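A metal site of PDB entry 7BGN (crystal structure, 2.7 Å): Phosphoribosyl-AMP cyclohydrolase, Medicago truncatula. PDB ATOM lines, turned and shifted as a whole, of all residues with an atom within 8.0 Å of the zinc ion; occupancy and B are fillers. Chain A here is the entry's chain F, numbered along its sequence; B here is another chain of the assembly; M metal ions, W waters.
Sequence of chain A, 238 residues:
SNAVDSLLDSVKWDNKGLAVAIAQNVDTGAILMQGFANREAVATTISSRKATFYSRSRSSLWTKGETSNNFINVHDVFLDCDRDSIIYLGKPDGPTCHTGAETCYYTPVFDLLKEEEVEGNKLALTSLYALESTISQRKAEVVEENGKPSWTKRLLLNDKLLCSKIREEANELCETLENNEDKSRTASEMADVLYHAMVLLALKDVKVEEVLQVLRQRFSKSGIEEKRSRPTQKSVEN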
ATOM      1  N   LYS A 165      26.136  -0.192  17.024  1.00  0.00           N
ATOM      2  CA  LYS A 165      25.533   1.130  16.930  1.00  0.00           C
ATOM      3  C   LYS A 165      24.708   1.245  15.660  1.00  0.00           C
ATOM      4  O   LYS A 165      23.653   1.896  15.659  1.00  0.00           O
ATOM      5  CB  LYS A 165      26.616   2.207  16.996  1.00  0.00           C
ATOM      6  CG  LYS A 165      26.599   3.050  18.291  1.00  0.00           C
ATOM      7  CD  LYS A 165      25.246   3.748  18.503  1.00  0.00           C
ATOM      8  CE  LYS A 165      25.293   4.769  19.639  1.00  0.00           C
ATOM      9  NZ  LYS A 165      23.941   5.184  20.167  1.00  0.00           N
ATOM     10  N   GLU A 168      21.626  -0.637  16.449  1.00  0.00           N
ATOM     11  CA  GLU A 168      20.829   0.118  17.418  1.00  0.00           C
ATOM     12  C   GLU A 168      20.091   1.262  16.746  1.00  0.00           C
ATOM     13  O   GLU A 168      18.898   1.476  16.985  1.00  0.00           O
ATOM     14  CB  GLU A 168      21.743   0.669  18.505  1.00  0.00           C
ATOM     15  CG  GLU A 168      21.116   1.809  19.287  1.00  0.00           C
ATOM     16  CD  GLU A 168      22.115   2.548  20.149  1.00  0.00           C
ATOM     17  OE1 GLU A 168      23.207   1.975  20.382  1.00  0.00           O
ATOM     18  OE2 GLU A 168      21.833   3.694  20.574  1.00  0.00           O
ATOM     19  N   GLU A 169      20.784   2.005  15.875  1.00  0.00           N
ATOM     20  CA  GLU A 169      20.161   3.184  15.284  1.00  0.00           C
ATOM     21  C   GLU A 169      19.093   2.812  14.252  1.00  0.00           C
ATOM     22  O   GLU A 169      18.096   3.515  14.121  1.00  0.00           O
ATOM     23  CB  GLU A 169      21.232   4.099  14.699  1.00  0.00           C
ATOM     24  CG  GLU A 169      22.197   4.644  15.776  1.00  0.00           C
ATOM     25  CD  GLU A 169      21.557   5.597  16.792  1.00  0.00           C
ATOM     26  OE1 GLU A 169      20.347   5.837  16.731  1.00  0.00           O
ATOM     27  OE2 GLU A 169      22.271   6.060  17.695  1.00  0.00           O
ATOM     28  N   ALA A 170      19.293   1.725  13.506  1.00  0.00           N
ATOM     29  CA  ALA A 170      18.251   1.260  12.596  1.00  0.00           C
ATOM     30  C   ALA A 170      16.981   0.898  13.357  1.00  0.00           C
ATOM     31  O   ALA A 170      15.858   1.099  12.881  1.00  0.00           O
ATOM     32  CB  ALA A 170      18.733   0.073  11.772  1.00  0.00           C
ATOM     33  N   ASN A 171      17.159   0.325  14.554  1.00  0.00           N
ATOM     34  CA  ASN A 171      16.024   0.041  15.419  1.00  0.00           C
ATOM     35  C   ASN A 171      15.276   1.311  15.789  1.00  0.00           C
ATOM     36  O   ASN A 171      14.045   1.375  15.676  1.00  0.00           O
ATOM     37  CB  ASN A 171      16.523  -0.669  16.666  1.00  0.00           C
ATOM     38  CG  ASN A 171      15.415  -1.071  17.570  1.00  0.00           C
ATOM     39  OD1 ASN A 171      14.302  -1.385  17.127  1.00  0.00           O
ATOM     40  ND2 ASN A 171      15.687  -1.048  18.862  1.00  0.00           N
ATOM     41  N   GLU A 172      16.015   2.351  16.201  1.00  0.00           N
ATOM     42  CA  GLU A 172      15.385   3.584  16.660  1.00  0.00           C
ATOM     43  C   GLU A 172      14.594   4.247  15.530  1.00  0.00           C
ATOM     44  O   GLU A 172      13.487   4.761  15.746  1.00  0.00           O
ATOM     45  CB  GLU A 172      16.449   4.534  17.211  1.00  0.00           C
ATOM     46  CG  GLU A 172      17.021   4.135  18.570  1.00  0.00           C
ATOM     47  CD  GLU A 172      18.329   4.884  18.920  1.00  0.00           C
ATOM     48  OE1 GLU A 172      18.685   5.876  18.237  1.00  0.00           O
ATOM     49  OE2 GLU A 172      19.011   4.457  19.876  1.00  0.00           O
ATOM     50  N   LEU A 173      15.136   4.187  14.304  1.00  0.00           N
ATOM     51  CA  LEU A 173      14.452   4.741  13.128  1.00  0.00           C
ATOM     52  C   LEU A 173      13.094   4.068  12.895  1.00  0.00           C
ATOM     53  O   LEU A 173      12.088   4.749  12.681  1.00  0.00           O
ATOM     54  CB  LEU A 173      15.364   4.594  11.910  1.00  0.00           C
ATOM     55  CG  LEU A 173      14.807   5.057  10.564  1.00  0.00           C
ATOM     56  CD1 LEU A 173      14.627   6.563  10.531  1.00  0.00           C
ATOM     57  CD2 LEU A 173      15.707   4.609   9.428  1.00  0.00           C
ATOM     58  N   THR A 176      10.388   5.055  15.323  1.00  0.00           N
ATOM     59  CA  THR A 176       9.714   6.319  15.047  1.00  0.00           C
ATOM     60  C   THR A 176       8.507   6.130  14.140  1.00  0.00           C
ATOM     61  O   THR A 176       7.532   6.888  14.258  1.00  0.00           O
ATOM     62  CB  THR A 176      10.693   7.331  14.436  1.00  0.00           C
ATOM     63  OG1 THR A 176      11.084   6.886  13.132  1.00  0.00           O
ATOM     64  CG2 THR A 176      11.922   7.489  15.309  1.00  0.00           C
ATOM     65  N   ARG A 185      11.860  13.311  14.783  1.00  0.00           N
ATOM     66  CA  ARG A 185      12.492  12.133  15.338  1.00  0.00           C
ATOM     67  C   ARG A 185      12.924  11.186  14.234  1.00  0.00           C
ATOM     68  O   ARG A 185      14.019  10.612  14.289  1.00  0.00           O
ATOM     69  CB  ARG A 185      11.535  11.429  16.307  1.00  0.00           C
ATOM     70  CG  ARG A 185      11.300  12.162  17.627  1.00  0.00           C
ATOM     71  CD  ARG A 185      12.564  12.206  18.453  1.00  0.00           C
ATOM     72  NE  ARG A 185      13.156  10.882  18.569  1.00  0.00           N
ATOM     73  CZ  ARG A 185      14.461  10.655  18.616  1.00  0.00           C
ATOM     74  NH1 ARG A 185      15.312  11.682  18.574  1.00  0.00           N
ATOM     75  NH2 ARG A 185      14.916   9.409  18.711  1.00  0.00           N
ATOM     76  N   SER A 188      15.843  12.858  12.623  1.00  0.00           N
ATOM     77  CA  SER A 188      16.996  12.765  13.507  1.00  0.00           C
ATOM     78  C   SER A 188      17.544  11.346  13.543  1.00  0.00           C
ATOM     79  O   SER A 188      18.761  11.152  13.514  1.00  0.00           O
ATOM     80  CB  SER A 188      16.630  13.209  14.915  1.00  0.00           C
ATOM     81  OG  SER A 188      17.746  13.047  15.766  1.00  0.00           O
ATOM     82  N   GLU A 189      16.666  10.338  13.570  1.00  0.00           N
ATOM     83  CA  GLU A 189      17.165   8.971  13.640  1.00  0.00           C
ATOM     84  C   GLU A 189      17.719   8.529  12.297  1.00  0.00           C
ATOM     85  O   GLU A 189      18.656   7.723  12.251  1.00  0.00           O
ATOM     86  CB  GLU A 189      16.068   8.010  14.097  1.00  0.00           C
ATOM     87  CG  GLU A 189      15.680   8.166  15.545  1.00  0.00           C
ATOM     88  CD  GLU A 189      16.879   8.276  16.453  1.00  0.00           C
ATOM     89  OE1 GLU A 189      17.772   7.408  16.417  1.00  0.00           O
ATOM     90  OE2 GLU A 189      16.915   9.265  17.230  1.00  0.00           O
ATOM     91  N   MET A 190      17.158   9.022  11.191  1.00  0.00           N
ATOM     92  CA  MET A 190      17.733   8.712   9.890  1.00  0.00           C
ATOM     93  C   MET A 190      19.151   9.256   9.763  1.00  0.00           C
ATOM     94  O   MET A 190      20.036   8.590   9.207  1.00  0.00           O
ATOM     95  CB  MET A 190      16.847   9.267   8.777  1.00  0.00           C
ATOM     96  CG  MET A 190      17.355   8.946   7.382  1.00  0.00           C
ATOM     97  SD  MET A 190      17.492   7.170   7.098  1.00  0.00           S
ATOM     98  CE  MET A 190      18.394   7.126   5.562  1.00  0.00           C
ATOM     99  N   ALA A 191      19.397  10.454  10.298  1.00  0.00           N
ATOM    100  CA  ALA A 191      20.748  10.993  10.311  1.00  0.00           C
ATOM    101  C   ALA A 191      21.676  10.127  11.148  1.00  0.00           C
ATOM    102  O   ALA A 191      22.849   9.932  10.794  1.00  0.00           O
ATOM    103  CB  ALA A 191      20.739  12.428  10.844  1.00  0.00           C
ATOM    104  N   ASP A 192      21.177   9.612  12.274  1.00  0.00           N
ATOM    105  CA  ASP A 192      21.958   8.681  13.092  1.00  0.00           C
ATOM    106  C   ASP A 192      22.305   7.433  12.304  1.00  0.00           C
ATOM    107  O   ASP A 192      23.425   6.918  12.407  1.00  0.00           O
ATOM    108  CB  ASP A 192      21.175   8.295  14.359  1.00  0.00           C
ATOM    109  CG  ASP A 192      21.105   9.403  15.393  1.00  0.00           C
ATOM    110  OD1 ASP A 192      21.646  10.507  15.128  1.00  0.00           O
ATOM    111  OD2 ASP A 192      20.515   9.180  16.481  1.00  0.00           O
ATOM    112  N   VAL A 193      21.367   6.908  11.515  1.00  0.00           N
ATOM    113  CA  VAL A 193      21.655   5.723  10.716  1.00  0.00           C
ATOM    114  C   VAL A 193      22.695   6.032   9.641  1.00  0.00           C
ATOM    115  O   VAL A 193      23.685   5.303   9.483  1.00  0.00           O
ATOM    116  CB  VAL A 193      20.358   5.166  10.096  1.00  0.00           C
ATOM    117  CG1 VAL A 193      20.688   4.108   9.097  1.00  0.00           C
ATOM    118  CG2 VAL A 193      19.488   4.597  11.195  1.00  0.00           C
ATOM    119  N   HIS A 196      26.549   6.464  11.051  1.00  0.00           N
ATOM    120  CA  HIS A 196      27.251   5.254  11.461  1.00  0.00           C
ATOM    121  C   HIS A 196      27.474   4.301  10.300  1.00  0.00           C
ATOM    122  O   HIS A 196      28.514   3.640  10.254  1.00  0.00           O
ATOM    123  CB  HIS A 196      26.479   4.572  12.587  1.00  0.00           C
ATOM    124  CG  HIS A 196      26.487   5.343  13.866  1.00  0.00           C
ATOM    125  ND1 HIS A 196      25.502   6.251  14.190  1.00  0.00           N
ATOM    126  CD2 HIS A 196      27.376   5.374  14.889  1.00  0.00           C
ATOM    127  CE1 HIS A 196      25.774   6.799  15.368  1.00  0.00           C
ATOM    128  NE2 HIS A 196      26.908   6.284  15.806  1.00  0.00           N
ATOM    129  N   ARG B 218      25.155  19.335  12.410  1.00  0.00           N
ATOM    130  CA  ARG B 218      25.991  18.708  13.434  1.00  0.00           C
ATOM    131  C   ARG B 218      27.491  18.907  13.188  1.00  0.00           C
ATOM    132  O   ARG B 218      28.294  18.290  13.872  1.00  0.00           O
ATOM    133  CB  ARG B 218      25.663  17.217  13.527  1.00  0.00           C
ATOM    134  CG  ARG B 218      24.245  16.926  14.005  1.00  0.00           C
ATOM    135  CD  ARG B 218      23.984  15.426  14.023  1.00  0.00           C
ATOM    136  NE  ARG B 218      22.587  15.085  14.299  1.00  0.00           N
ATOM    137  CZ  ARG B 218      22.092  13.850  14.162  1.00  0.00           C
ATOM    138  NH1 ARG B 218      22.869  12.853  13.754  1.00  0.00           N
ATOM    139  NH2 ARG B 218      20.801  13.616  14.433  1.00  0.00           N
HETATM  140 ZN    ZN M   1      19.602   7.539  17.361  1.00  0.00          ZN
HETATM  141  O   HOH W   1      20.447   7.442  19.732  1.00  0.00           O
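The side-chain amino group (NZ) of Lys 165 is in salt-bridge range of the side-chain carboxylate (OE2) of Glu 169 (3.1 Å).
NH2 of Arg 185 is in salt-bridge range of OE2 of Glu 189, at 2.5 Å.
O of Asp 192 is in hydrogen-bond range of ND1 of His 196 (2.8 Å).
The side-chain carboxylate of Asp 192 lies within salt-bridge range of the guanidinium group of Arg 218 of chain B (3.0 Å).
Of the 17 residues printed, 4 come within 4 Å of the zinc ion.
The nearest printed residue that does not touch the zinc ion is Arg 185 (5.2 Å).
The zinc ion is bound by OE1 of Glu 169 (2.0 Å), OE1 of Glu 189 (2.1 Å), OD2 of Asp 192 (2.1 Å), OE1 of Glu 172 (2.1 Å) and water W1 (2.5 Å).
The zinc ion has five donor atoms within binding distance.
Water W1 lies within hydrogen-bond range of OE2 of Glu 169 (3.1 Å) and OE2 of Glu 172 (3.3 Å).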
